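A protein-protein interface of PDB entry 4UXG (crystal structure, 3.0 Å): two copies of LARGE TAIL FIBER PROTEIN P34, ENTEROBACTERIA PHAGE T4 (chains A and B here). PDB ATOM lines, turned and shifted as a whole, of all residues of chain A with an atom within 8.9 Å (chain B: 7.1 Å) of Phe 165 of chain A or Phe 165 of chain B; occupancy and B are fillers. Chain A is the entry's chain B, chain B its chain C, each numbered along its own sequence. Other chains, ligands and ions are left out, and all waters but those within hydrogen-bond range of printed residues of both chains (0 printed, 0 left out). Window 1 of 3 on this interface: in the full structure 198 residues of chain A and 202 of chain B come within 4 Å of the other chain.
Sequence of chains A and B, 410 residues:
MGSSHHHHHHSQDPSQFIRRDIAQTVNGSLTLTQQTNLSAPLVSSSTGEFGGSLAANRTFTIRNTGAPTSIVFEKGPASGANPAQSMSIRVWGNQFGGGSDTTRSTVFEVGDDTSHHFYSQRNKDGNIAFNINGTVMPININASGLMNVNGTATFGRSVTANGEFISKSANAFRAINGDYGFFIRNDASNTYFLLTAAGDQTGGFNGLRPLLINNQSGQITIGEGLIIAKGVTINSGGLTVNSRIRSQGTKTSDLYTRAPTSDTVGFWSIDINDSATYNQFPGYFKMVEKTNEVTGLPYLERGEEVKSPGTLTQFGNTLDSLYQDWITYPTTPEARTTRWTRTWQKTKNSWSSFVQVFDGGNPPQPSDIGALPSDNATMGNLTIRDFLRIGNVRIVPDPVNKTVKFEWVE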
ATOM      1  N   ALA A 153       1.448  16.396  -9.420  1.00  0.00           N
ATOM      2  CA  ALA A 153       0.643  15.689  -8.445  1.00  0.00           C
ATOM      3  C   ALA A 153      -0.529  15.038  -9.155  1.00  0.00           C
ATOM      4  O   ALA A 153      -1.114  15.622 -10.065  1.00  0.00           O
ATOM      5  CB  ALA A 153       0.158  16.630  -7.367  1.00  0.00           C
ATOM      6  N   THR A 154      -0.865  13.825  -8.736  1.00  0.00           N
ATOM      7  CA  THR A 154      -1.991  13.106  -9.307  1.00  0.00           C
ATOM      8  C   THR A 154      -2.859  12.534  -8.200  1.00  0.00           C
ATOM      9  O   THR A 154      -2.362  11.957  -7.234  1.00  0.00           O
ATOM     10  CB  THR A 154      -1.529  11.974 -10.230  1.00  0.00           C
ATOM     11  OG1 THR A 154      -0.636  11.115  -9.515  1.00  0.00           O
ATOM     12  CG2 THR A 154      -0.800  12.536 -11.431  1.00  0.00           C
ATOM     13  N   PHE A 155      -4.166  12.691  -8.364  1.00  0.00           N
ATOM     14  CA  PHE A 155      -5.133  12.246  -7.380  1.00  0.00           C
ATOM     15  C   PHE A 155      -6.102  11.276  -8.021  1.00  0.00           C
ATOM     16  O   PHE A 155      -6.527  11.470  -9.157  1.00  0.00           O
ATOM     17  CB  PHE A 155      -5.847  13.459  -6.794  1.00  0.00           C
ATOM     18  CG  PHE A 155      -4.989  14.265  -5.868  1.00  0.00           C
ATOM     19  CD1 PHE A 155      -4.447  13.692  -4.736  1.00  0.00           C
ATOM     20  CD2 PHE A 155      -4.635  15.562  -6.181  1.00  0.00           C
ATOM     21  CE1 PHE A 155      -3.640  14.421  -3.887  1.00  0.00           C
ATOM     22  CE2 PHE A 155      -3.814  16.293  -5.342  1.00  0.00           C
ATOM     23  CZ  PHE A 155      -3.319  15.720  -4.192  1.00  0.00           C
ATOM     24  N   GLY A 156      -6.446  10.224  -7.295  1.00  0.00           N
ATOM     25  CA  GLY A 156      -7.230   9.155  -7.871  1.00  0.00           C
ATOM     26  C   GLY A 156      -8.715   9.326  -7.693  1.00  0.00           C
ATOM     27  O   GLY A 156      -9.500   8.670  -8.370  1.00  0.00           O
ATOM     28  N   ARG A 157      -9.101  10.212  -6.782  1.00  0.00           N
ATOM     29  CA  ARG A 157     -10.514  10.482  -6.532  1.00  0.00           C
ATOM     30  C   ARG A 157     -10.714  11.982  -6.293  1.00  0.00           C
ATOM     31  O   ARG A 157     -10.057  12.802  -6.922  1.00  0.00           O
ATOM     32  CB  ARG A 157     -11.018   9.644  -5.353  1.00  0.00           C
ATOM     33  CG  ARG A 157     -10.959   8.137  -5.614  1.00  0.00           C
ATOM     34  CD  ARG A 157     -11.492   7.310  -4.457  1.00  0.00           C
ATOM     35  NE  ARG A 157     -12.935   7.423  -4.281  1.00  0.00           N
ATOM     36  CZ  ARG A 157     -13.595   6.922  -3.243  1.00  0.00           C
ATOM     37  NH1 ARG A 157     -12.936   6.286  -2.282  1.00  0.00           N
ATOM     38  NH2 ARG A 157     -14.910   7.065  -3.155  1.00  0.00           N
ATOM     39  N   SER A 158     -11.623  12.352  -5.402  1.00  0.00           N
ATOM     40  CA  SER A 158     -11.915  13.763  -5.199  1.00  0.00           C
ATOM     41  C   SER A 158     -10.844  14.472  -4.378  1.00  0.00           C
ATOM     42  O   SER A 158     -10.070  13.845  -3.665  1.00  0.00           O
ATOM     43  CB  SER A 158     -13.276  13.944  -4.526  1.00  0.00           C
ATOM     44  OG  SER A 158     -13.332  13.291  -3.274  1.00  0.00           O
ATOM     45  N   VAL A 159     -10.802  15.790  -4.510  1.00  0.00           N
ATOM     46  CA  VAL A 159      -9.910  16.633  -3.740  1.00  0.00           C
ATOM     47  C   VAL A 159     -10.712  17.776  -3.142  1.00  0.00           C
ATOM     48  O   VAL A 159     -11.235  18.609  -3.866  1.00  0.00           O
ATOM     49  CB  VAL A 159      -8.783  17.196  -4.605  1.00  0.00           C
ATOM     50  CG1 VAL A 159      -7.881  18.090  -3.786  1.00  0.00           C
ATOM     51  CG2 VAL A 159      -8.003  16.073  -5.252  1.00  0.00           C
ATOM     52  N   THR A 160     -10.829  17.801  -1.823  1.00  0.00           N
ATOM     53  CA  THR A 160     -11.645  18.801  -1.140  1.00  0.00           C
ATOM     54  C   THR A 160     -10.798  19.698  -0.246  1.00  0.00           C
ATOM     55  O   THR A 160     -10.042  19.206   0.586  1.00  0.00           O
ATOM     56  CB  THR A 160     -12.747  18.135  -0.291  1.00  0.00           C
ATOM     57  OG1 THR A 160     -13.582  17.337  -1.136  1.00  0.00           O
ATOM     58  CG2 THR A 160     -13.603  19.175   0.400  1.00  0.00           C
ATOM     59  N   ALA A 161     -10.939  21.009  -0.403  1.00  0.00           N
ATOM     60  CA  ALA A 161     -10.214  21.957   0.438  1.00  0.00           C
ATOM     61  C   ALA A 161     -11.156  22.892   1.163  1.00  0.00           C
ATOM     62  O   ALA A 161     -12.090  23.415   0.570  1.00  0.00           O
ATOM     63  CB  ALA A 161      -9.233  22.758  -0.390  1.00  0.00           C
ATOM     64  N   ASN A 162     -10.899  23.113   2.448  1.00  0.00           N
ATOM     65  CA  ASN A 162     -11.648  24.102   3.211  1.00  0.00           C
ATOM     66  C   ASN A 162     -11.227  25.498   2.789  1.00  0.00           C
ATOM     67  O   ASN A 162     -11.866  26.482   3.142  1.00  0.00           O
ATOM     68  CB  ASN A 162     -11.432  23.930   4.713  1.00  0.00           C
ATOM     69  CG  ASN A 162     -12.011  22.639   5.248  1.00  0.00           C
ATOM     70  OD1 ASN A 162     -12.866  22.019   4.619  1.00  0.00           O
ATOM     71  ND2 ASN A 162     -11.551  22.232   6.426  1.00  0.00           N
ATOM     72  N   GLY A 163     -10.128  25.576   2.054  1.00  0.00           N
ATOM     73  CA  GLY A 163      -9.640  26.849   1.579  1.00  0.00           C
ATOM     74  C   GLY A 163      -9.794  26.997   0.084  1.00  0.00           C
ATOM     75  O   GLY A 163     -10.528  26.255  -0.556  1.00  0.00           O
ATOM     76  N   GLU A 164      -9.066  27.958  -0.467  1.00  0.00           N
ATOM     77  CA  GLU A 164      -9.171  28.346  -1.866  1.00  0.00           C
ATOM     78  C   GLU A 164      -8.251  27.517  -2.756  1.00  0.00           C
ATOM     79  O   GLU A 164      -7.144  27.170  -2.357  1.00  0.00           O
ATOM     80  CB  GLU A 164      -8.847  29.842  -1.994  1.00  0.00           C
ATOM     81  CG  GLU A 164      -9.259  30.519  -3.287  1.00  0.00           C
ATOM     82  CD  GLU A 164      -8.989  32.020  -3.261  1.00  0.00           C
ATOM     83  OE1 GLU A 164      -8.439  32.510  -2.250  1.00  0.00           O
ATOM     84  OE2 GLU A 164      -9.335  32.714  -4.245  1.00  0.00           O
ATOM     85  N   PHE A 165      -8.713  27.194  -3.958  1.00  0.00           N
ATOM     86  CA  PHE A 165      -7.834  26.628  -4.972  1.00  0.00           C
ATOM     87  C   PHE A 165      -7.236  27.764  -5.787  1.00  0.00           C
ATOM     88  O   PHE A 165      -7.955  28.626  -6.271  1.00  0.00           O
ATOM     89  CB  PHE A 165      -8.587  25.652  -5.872  1.00  0.00           C
ATOM     90  CG  PHE A 165      -8.886  24.341  -5.218  1.00  0.00           C
ATOM     91  CD1 PHE A 165     -10.020  24.179  -4.447  1.00  0.00           C
ATOM     92  CD2 PHE A 165      -8.031  23.270  -5.371  1.00  0.00           C
ATOM     93  CE1 PHE A 165     -10.296  22.969  -3.842  1.00  0.00           C
ATOM     94  CE2 PHE A 165      -8.306  22.063  -4.773  1.00  0.00           C
ATOM     95  CZ  PHE A 165      -9.438  21.914  -4.005  1.00  0.00           C
ATOM     96  N   ILE A 166      -5.914  27.781  -5.907  1.00  0.00           N
ATOM     97  CA  ILE A 166      -5.232  28.866  -6.595  1.00  0.00           C
ATOM     98  C   ILE A 166      -4.226  28.356  -7.616  1.00  0.00           C
ATOM     99  O   ILE A 166      -3.389  27.513  -7.309  1.00  0.00           O
ATOM    100  CB  ILE A 166      -4.516  29.774  -5.594  1.00  0.00           C
ATOM    101  CG1 ILE A 166      -5.517  30.323  -4.575  1.00  0.00           C
ATOM    102  CG2 ILE A 166      -3.802  30.896  -6.316  1.00  0.00           C
ATOM    103  CD1 ILE A 166      -4.883  30.762  -3.293  1.00  0.00           C
ATOM    104  N   SER A 167      -4.323  28.868  -8.836  1.00  0.00           N
ATOM    105  CA  SER A 167      -3.375  28.547  -9.893  1.00  0.00           C
ATOM    106  C   SER A 167      -2.635  29.786 -10.358  1.00  0.00           C
ATOM    107  O   SER A 167      -3.222  30.856 -10.492  1.00  0.00           O
ATOM    108  CB  SER A 167      -4.083  27.901 -11.080  1.00  0.00           C
ATOM    109  OG  SER A 167      -3.186  27.726 -12.162  1.00  0.00           O
ATOM    110  N   LYS A 168      -1.340  29.635 -10.602  1.00  0.00           N
ATOM    111  CA  LYS A 168      -0.531  30.724 -11.120  1.00  0.00           C
ATOM    112  C   LYS A 168      -0.189  30.475 -12.577  1.00  0.00           C
ATOM    113  O   LYS A 168       0.615  31.193 -13.169  1.00  0.00           O
ATOM    114  CB  LYS A 168       0.728  30.910 -10.280  1.00  0.00           C
ATOM    115  CG  LYS A 168       0.433  31.234  -8.821  1.00  0.00           C
ATOM    116  CD  LYS A 168       1.687  31.657  -8.081  1.00  0.00           C
ATOM    117  CE  LYS A 168       1.358  32.229  -6.714  1.00  0.00           C
ATOM    118  NZ  LYS A 168       2.600  32.584  -5.970  1.00  0.00           N
ATOM    119  N   ALA A 172      -5.541  27.709 -16.014  1.00  0.00           N
ATOM    120  CA  ALA A 172      -5.616  27.507 -14.575  1.00  0.00           C
ATOM    121  C   ALA A 172      -6.473  26.326 -14.140  1.00  0.00           C
ATOM    122  O   ALA A 172      -6.084  25.571 -13.256  1.00  0.00           O
ATOM    123  CB  ALA A 172      -6.126  28.763 -13.929  1.00  0.00           C
ATOM    124  N   PHE A 173      -7.652  26.185 -14.729  1.00  0.00           N
ATOM    125  CA  PHE A 173      -8.580  25.139 -14.321  1.00  0.00           C
ATOM    126  C   PHE A 173      -9.147  24.437 -15.538  1.00  0.00           C
ATOM    127  O   PHE A 173      -9.673  25.080 -16.427  1.00  0.00           O
ATOM    128  CB  PHE A 173      -9.708  25.716 -13.477  1.00  0.00           C
ATOM    129  CG  PHE A 173      -9.239  26.365 -12.209  1.00  0.00           C
ATOM    130  CD1 PHE A 173      -8.915  27.706 -12.183  1.00  0.00           C
ATOM    131  CD2 PHE A 173      -9.128  25.634 -11.040  1.00  0.00           C
ATOM    132  CE1 PHE A 173      -8.484  28.307 -11.013  1.00  0.00           C
ATOM    133  CE2 PHE A 173      -8.704  26.232  -9.870  1.00  0.00           C
ATOM    134  CZ  PHE A 173      -8.382  27.570  -9.857  1.00  0.00           C
ATOM    135  N   ARG A 174      -9.043  23.117 -15.579  1.00  0.00           N
ATOM    136  CA  ARG A 174      -9.468  22.371 -16.752  1.00  0.00           C
ATOM    137  C   ARG A 174     -10.363  21.192 -16.409  1.00  0.00           C
ATOM    138  O   ARG A 174     -10.110  20.448 -15.465  1.00  0.00           O
ATOM    139  CB  ARG A 174      -8.248  21.894 -17.536  1.00  0.00           C
ATOM    140  CG  ARG A 174      -8.580  21.084 -18.767  1.00  0.00           C
ATOM    141  CD  ARG A 174      -7.329  20.724 -19.520  1.00  0.00           C
ATOM    142  NE  ARG A 174      -6.644  21.920 -19.988  1.00  0.00           N
ATOM    143  CZ  ARG A 174      -6.294  22.134 -21.252  1.00  0.00           C
ATOM    144  NH1 ARG A 174      -6.549  21.222 -22.175  1.00  0.00           N
ATOM    145  NH2 ARG A 174      -5.674  23.254 -21.591  1.00  0.00           N
ATOM    146  N   ALA A 175     -11.432  21.057 -17.183  1.00  0.00           N
ATOM    147  CA  ALA A 175     -12.352  19.937 -17.085  1.00  0.00           C
ATOM    148  C   ALA A 175     -12.281  19.121 -18.367  1.00  0.00           C
ATOM    149  O   ALA A 175     -12.584  19.627 -19.446  1.00  0.00           O
ATOM    150  CB  ALA A 175     -13.761  20.425 -16.838  1.00  0.00           C
ATOM    151  N   VAL B 159      -1.692  19.765 -11.098  1.00  0.00           N
ATOM    152  CA  VAL B 159      -2.401  18.934 -10.136  1.00  0.00           C
ATOM    153  C   VAL B 159      -3.588  18.311 -10.850  1.00  0.00           C
ATOM    154  O   VAL B 159      -4.495  19.018 -11.279  1.00  0.00           O
ATOM    155  CB  VAL B 159      -2.885  19.743  -8.932  1.00  0.00           C
ATOM    156  CG1 VAL B 159      -3.613  18.849  -7.945  1.00  0.00           C
ATOM    157  CG2 VAL B 159      -1.717  20.445  -8.271  1.00  0.00           C
ATOM    158  N   THR B 160      -3.567  16.990 -10.992  1.00  0.00           N
ATOM    159  CA  THR B 160      -4.574  16.281 -11.777  1.00  0.00           C
ATOM    160  C   THR B 160      -5.400  15.340 -10.904  1.00  0.00           C
ATOM    161  O   THR B 160      -4.842  14.565 -10.128  1.00  0.00           O
ATOM    162  CB  THR B 160      -3.920  15.468 -12.901  1.00  0.00           C
ATOM    163  OG1 THR B 160      -3.066  16.313 -13.679  1.00  0.00           O
ATOM    164  CG2 THR B 160      -4.971  14.826 -13.783  1.00  0.00           C
ATOM    165  N   ALA B 161      -6.723  15.420 -11.011  1.00  0.00           N
ATOM    166  CA  ALA B 161      -7.595  14.519 -10.260  1.00  0.00           C
ATOM    167  C   ALA B 161      -8.562  13.747 -11.152  1.00  0.00           C
ATOM    168  O   ALA B 161      -9.165  14.317 -12.051  1.00  0.00           O
ATOM    169  CB  ALA B 161      -8.370  15.292  -9.209  1.00  0.00           C
ATOM    170  N   ASN B 162      -8.712  12.451 -10.896  1.00  0.00           N
ATOM    171  CA  ASN B 162      -9.728  11.662 -11.584  1.00  0.00           C
ATOM    172  C   ASN B 162     -11.104  12.009 -11.051  1.00  0.00           C
ATOM    173  O   ASN B 162     -12.123  11.662 -11.642  1.00  0.00           O
ATOM    174  CB  ASN B 162      -9.473  10.162 -11.423  1.00  0.00           C
ATOM    175  CG  ASN B 162      -8.221   9.699 -12.139  1.00  0.00           C
ATOM    176  OD1 ASN B 162      -7.728  10.366 -13.047  1.00  0.00           O
ATOM    177  ND2 ASN B 162      -7.696   8.551 -11.727  1.00  0.00           N
ATOM    178  N   GLY B 163     -11.125  12.682  -9.911  1.00  0.00           N
ATOM    179  CA  GLY B 163     -12.368  13.090  -9.300  1.00  0.00           C
ATOM    180  C   GLY B 163     -12.564  14.588  -9.312  1.00  0.00           C
ATOM    181  O   GLY B 163     -11.875  15.320 -10.015  1.00  0.00           O
ATOM    182  N   GLU B 164     -13.485  15.033  -8.469  1.00  0.00           N
ATOM    183  CA  GLU B 164     -13.923  16.416  -8.411  1.00  0.00           C
ATOM    184  C   GLU B 164     -13.033  17.244  -7.491  1.00  0.00           C
ATOM    185  O   GLU B 164     -12.623  16.776  -6.437  1.00  0.00           O
ATOM    186  CB  GLU B 164     -15.374  16.449  -7.914  1.00  0.00           C
ATOM    187  CG  GLU B 164     -16.155  17.727  -8.129  1.00  0.00           C
ATOM    188  CD  GLU B 164     -17.596  17.588  -7.653  1.00  0.00           C
ATOM    189  OE1 GLU B 164     -17.937  16.515  -7.113  1.00  0.00           O
ATOM    190  OE2 GLU B 164     -18.390  18.540  -7.821  1.00  0.00           O
ATOM    191  N   PHE B 165     -12.755  18.482  -7.879  1.00  0.00           N
ATOM    192  CA  PHE B 165     -12.144  19.439  -6.969  1.00  0.00           C
ATOM    193  C   PHE B 165     -13.265  20.173  -6.254  1.00  0.00           C
ATOM    194  O   PHE B 165     -14.166  20.702  -6.895  1.00  0.00           O
ATOM    195  CB  PHE B 165     -11.261  20.430  -7.716  1.00  0.00           C
ATOM    196  CG  PHE B 165      -9.967  19.856  -8.194  1.00  0.00           C
ATOM    197  CD1 PHE B 165      -8.844  19.893  -7.399  1.00  0.00           C
ATOM    198  CD2 PHE B 165      -9.867  19.303  -9.451  1.00  0.00           C
ATOM    199  CE1 PHE B 165      -7.654  19.378  -7.848  1.00  0.00           C
ATOM    200  CE2 PHE B 165      -8.677  18.792  -9.904  1.00  0.00           C
ATOM    201  CZ  PHE B 165      -7.574  18.827  -9.103  1.00  0.00           C
ATOM    202  N   ILE B 166     -13.220  20.211  -4.931  1.00  0.00           N
ATOM    203  CA  ILE B 166     -14.296  20.829  -4.166  1.00  0.00           C
ATOM    204  C   ILE B 166     -13.736  21.835  -3.176  1.00  0.00           C
ATOM    205  O   ILE B 166     -12.814  21.530  -2.421  1.00  0.00           O
ATOM    206  CB  ILE B 166     -15.113  19.784  -3.400  1.00  0.00           C
ATOM    207  CG1 ILE B 166     -15.616  18.695  -4.348  1.00  0.00           C
ATOM    208  CG2 ILE B 166     -16.245  20.456  -2.636  1.00  0.00           C
ATOM    209  CD1 ILE B 166     -15.948  17.406  -3.653  1.00  0.00           C
ATOM    210  N   SER B 167     -14.290  23.037  -3.182  1.00  0.00           N
ATOM    211  CA  SER B 167     -13.879  24.056  -2.230  1.00  0.00           C
ATOM    212  C   SER B 167     -15.019  24.443  -1.320  1.00  0.00           C
ATOM    213  O   SER B 167     -16.154  24.562  -1.759  1.00  0.00           O
ATOM    214  CB  SER B 167     -13.356  25.290  -2.954  1.00  0.00           C
ATOM    215  OG  SER B 167     -13.081  26.322  -2.029  1.00  0.00           O
ATOM    216  N   LYS B 168     -14.714  24.633  -0.045  1.00  0.00           N
ATOM    217  CA  LYS B 168     -15.719  25.060   0.911  1.00  0.00           C
ATOM    218  C   LYS B 168     -15.501  26.515   1.277  1.00  0.00           C
ATOM    219  O   LYS B 168     -16.183  27.064   2.137  1.00  0.00           O
ATOM    220  CB  LYS B 168     -15.697  24.171   2.156  1.00  0.00           C
ATOM    221  CG  LYS B 168     -15.965  22.702   1.853  1.00  0.00           C
ATOM    222  CD  LYS B 168     -16.216  21.902   3.115  1.00  0.00           C
ATOM    223  CE  LYS B 168     -16.756  20.519   2.784  1.00  0.00           C
ATOM    224  NZ  LYS B 168     -16.967  19.697   4.009  1.00  0.00           N
ATOM    225  N   SER B 169     -14.573  27.146   0.573  1.00  0.00           N
ATOM    226  CA  SER B 169     -14.311  28.556   0.762  1.00  0.00           C
ATOM    227  C   SER B 169     -15.257  29.373  -0.088  1.00  0.00           C
ATOM    228  O   SER B 169     -15.638  28.944  -1.180  1.00  0.00           O
ATOM    229  CB  SER B 169     -12.869  28.881   0.390  1.00  0.00           C
ATOM    230  OG  SER B 169     -12.637  30.275   0.440  1.00  0.00           O
ATOM    231  N   ASN B 171     -14.539  32.310  -1.593  1.00  0.00           N
ATOM    232  CA  ASN B 171     -13.669  32.391  -2.755  1.00  0.00           C
ATOM    233  C   ASN B 171     -13.085  31.009  -3.006  1.00  0.00           C
ATOM    234  O   ASN B 171     -12.212  30.555  -2.268  1.00  0.00           O
ATOM    235  CB  ASN B 171     -12.563  33.424  -2.556  1.00  0.00           C
ATOM    236  CG  ASN B 171     -13.110  34.810  -2.307  1.00  0.00           C
ATOM    237  OD1 ASN B 171     -14.305  35.042  -2.438  1.00  0.00           O
ATOM    238  ND2 ASN B 171     -12.235  35.746  -1.970  1.00  0.00           N
ATOM    239  N   ALA B 172     -13.565  30.343  -4.051  1.00  0.00           N
ATOM    240  CA  ALA B 172     -13.310  28.919  -4.225  1.00  0.00           C
ATOM    241  C   ALA B 172     -12.193  28.596  -5.212  1.00  0.00           C
ATOM    242  O   ALA B 172     -11.353  27.747  -4.933  1.00  0.00           O
ATOM    243  CB  ALA B 172     -14.569  28.242  -4.651  1.00  0.00           C
ATOM    244  N   PHE B 173     -12.185  29.257  -6.362  1.00  0.00           N
ATOM    245  CA  PHE B 173     -11.215  28.951  -7.409  1.00  0.00           C
ATOM    246  C   PHE B 173     -10.604  30.226  -7.953  1.00  0.00           C
ATOM    247  O   PHE B 173     -11.320  31.128  -8.354  1.00  0.00           O
ATOM    248  CB  PHE B 173     -11.871  28.171  -8.546  1.00  0.00           C
ATOM    249  CG  PHE B 173     -12.456  26.862  -8.121  1.00  0.00           C
ATOM    250  CD1 PHE B 173     -11.686  25.716  -8.107  1.00  0.00           C
ATOM    251  CD2 PHE B 173     -13.782  26.778  -7.739  1.00  0.00           C
ATOM    252  CE1 PHE B 173     -12.227  24.512  -7.716  1.00  0.00           C
ATOM    253  CE2 PHE B 173     -14.329  25.575  -7.345  1.00  0.00           C
ATOM    254  CZ  PHE B 173     -13.551  24.443  -7.334  1.00  0.00           C
ATOM    255  N   ARG B 174      -9.281  30.309  -7.976  1.00  0.00           N
ATOM    256  CA  ARG B 174      -8.635  31.538  -8.405  1.00  0.00           C
ATOM    257  C   ARG B 174      -7.553  31.287  -9.438  1.00  0.00           C
ATOM    258  O   ARG B 174      -6.745  30.374  -9.301  1.00  0.00           O
ATOM    259  CB  ARG B 174      -8.044  32.280  -7.204  1.00  0.00           C
ATOM    260  CG  ARG B 174      -7.344  33.589  -7.560  1.00  0.00           C
ATOM    261  CD  ARG B 174      -6.839  34.311  -6.326  1.00  0.00           C
ATOM    262  NE  ARG B 174      -7.946  34.647  -5.437  1.00  0.00           N
ATOM    263  CZ  ARG B 174      -8.199  35.867  -4.982  1.00  0.00           C
ATOM    264  NH1 ARG B 174      -7.415  36.877  -5.323  1.00  0.00           N
ATOM    265  NH2 ARG B 174      -9.234  36.078  -4.180  1.00  0.00           N
ATOM    266  N   ALA B 175      -7.562  32.107 -10.479  1.00  0.00           N
ATOM    267  CA  ALA B 175      -6.534  32.095 -11.500  1.00  0.00           C
ATOM    268  C   ALA B 175      -5.767  33.405 -11.430  1.00  0.00           C
ATOM    269  O   ALA B 175      -6.331  34.481 -11.639  1.00  0.00           O
ATOM    270  CB  ALA B 175      -7.140  31.905 -12.862  1.00  0.00           C
ATOM    271  N   PHE B 182      -8.384  36.483 -11.071  1.00  0.00           N
ATOM    272  CA  PHE B 182      -9.785  36.221 -11.382  1.00  0.00           C
ATOM    273  C   PHE B 182     -10.254  35.115 -10.456  1.00  0.00           C
ATOM    274  O   PHE B 182      -9.514  34.170 -10.232  1.00  0.00           O
ATOM    275  CB  PHE B 182      -9.925  35.802 -12.846  1.00  0.00           C
ATOM    276  CG  PHE B 182     -11.259  35.193 -13.201  1.00  0.00           C
ATOM    277  CD1 PHE B 182     -12.350  35.993 -13.496  1.00  0.00           C
ATOM    278  CD2 PHE B 182     -11.419  33.819 -13.244  1.00  0.00           C
ATOM    279  CE1 PHE B 182     -13.569  35.432 -13.835  1.00  0.00           C
ATOM    280  CE2 PHE B 182     -12.636  33.256 -13.575  1.00  0.00           C
ATOM    281  CZ  PHE B 182     -13.711  34.064 -13.870  1.00  0.00           C
ATOM    282  N   PHE B 183     -11.444  35.212  -9.876  1.00  0.00           N
ATOM    283  CA  PHE B 183     -11.872  34.095  -9.033  1.00  0.00           C
ATOM    284  C   PHE B 183     -13.373  33.894  -8.902  1.00  0.00           C
ATOM    285  O   PHE B 183     -14.158  34.817  -9.072  1.00  0.00           O
ATOM    286  CB  PHE B 183     -11.256  34.215  -7.637  1.00  0.00           C
ATOM    287  CG  PHE B 183     -11.615  35.465  -6.891  1.00  0.00           C
ATOM    288  CD1 PHE B 183     -10.918  36.642  -7.102  1.00  0.00           C
ATOM    289  CD2 PHE B 183     -12.609  35.446  -5.926  1.00  0.00           C
ATOM    290  CE1 PHE B 183     -11.229  37.785  -6.386  1.00  0.00           C
ATOM    291  CE2 PHE B 183     -12.925  36.587  -5.208  1.00  0.00           C
ATOM    292  CZ  PHE B 183     -12.233  37.757  -5.439  1.00  0.00           C
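Ala 161 of chain B touches Arg 157 of chain A.
Ser 158 of chain A touches Glu 164 of chain B.
CA of Thr 160 of chain A touches O of Ile 166 of chain B (3.2 Å).
Phe 165 of chain A touches Ile 166 of chain B.
CA of Phe 173 of chain B touches O of Phe 165 of chain A, 3.5 Å away.
Thr 160 of chain A touches Ile 166 of chain B, but with the chains exchanged Ile 166 of chain A does not touch Thr 160 of chain B (11.2 Å).
Of the 38 pairs that touch across the chains among the printed residues, 2 have their exchanged pair printed and touching as well.
N of Ser 167 of chain A is in hydrogen-bond range of O of Arg 174 of chain B, at 2.9 Å.
N of Ala 161 of chain A sits at hydrogen-bond distance from O of Ile 166 of chain B.
O of Glu 164 of chain B sits at hydrogen-bond distance from N of Val 159 of chain A, at 2.8 Å.
O of Ala 172 of chain B is in hydrogen-bond range of N of Phe 165 of chain A (2.9 Å).
N of Arg 174 of chain B sits at hydrogen-bond distance from O of Phe 165 of chain A (2.7 Å).
The backbone NH of Lys 168 of chain B sits at hydrogen-bond distance from the backbone carbonyl oxygen of Ala 161 of chain A (3.0 Å).
The backbone NH (N) of Phe 155 of chain A sits at hydrogen-bond distance from the backbone carbonyl oxygen (O) of Thr 160 of chain B (2.7 Å).
The backbone NH (N) of Asn 162 of chain B sits at hydrogen-bond distance from the backbone carbonyl oxygen (O) of Phe 155 of chain A.
N of Gly 163 of chain B sits at hydrogen-bond distance from O of Arg 157 of chain A.
O of Gly 163 of chain A is in hydrogen-bond range of OG of Ser 167 of chain B (2.9 Å).
The backbone NH (N) of Ile 166 of chain B is in hydrogen-bond range of the backbone carbonyl oxygen (O) of Val 159 of chain A, 2.8 Å away.
The backbone carbonyl oxygen (O) of Ala 153 of chain A sits at hydrogen-bond distance from the backbone NH (N) of Thr 160 of chain B (3.0 Å).
The side-chain carboxylate of Glu 164 of chain A lies within salt-bridge range of the guanidinium group of Arg 174 of chain B (2.7 Å).
Of the 18 printed residues of chain B, 16 touch a printed residue of chain A.
Printed residues of chain A that touch a printed residue of chain B: Ala 153, Thr 154, Phe 155, Gly 156, Arg 157, Ser 158, Val 159, Thr 160, Ala 161, Asn 162, Gly 163, Glu 164, Phe 165, Ile 166, Ser 167, Ala 172 and Phe 173.
Hydrophobic or aromatic side chains of chain A that line the printed part of chain B: Phe 155, Val 159, Phe 165, Ala 172 and Phe 173.
Among the printed residues, Asp or Glu carboxylates within 4 Å of a Lys or Arg side-chain nitrogen of the other chain: Glu 164 of chain A with Arg 174 of chain B (2.7 Å).
The backbone carbonyl oxygen of Asn 171 of chain B is in hydrogen-bond range of the side-chain hydroxyl of Ser 169 of chain B.
N of Ala 175 of chain B is in hydrogen-bond range of O of Phe 182 of chain B (2.9 Å).
Of chain B, only Phe 165 (3.4 Å), Ile 166 (3.2 Å), Ser 167 (3.8 Å), Ala 172 (2.9 Å), Phe 173 (3.5 Å) and Arg 174 (2.7 Å) come within 4 Å of Phe 165 of chain A.
Of chain A, only Val 159 (3.3 Å) and Phe 165 (3.4 Å) come within 4 Å of Phe 165 of chain B.
Printed residues of chain A within 4 Å of Ala 172 of chain B: Glu 164 and Phe 165.
Ala 175 of chain A touches none of the printed residues of chain B.
Phe 182 of chain B touches none of the printed residues of chain A.
The nearest residue of chain B that does not touch Phe 165 of chain A is Asn 171 of chain B (5.1 Å).
The nearest residue of chain A that does not touch Phe 165 of chain B is Phe 155 of chain A (5.1 Å).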
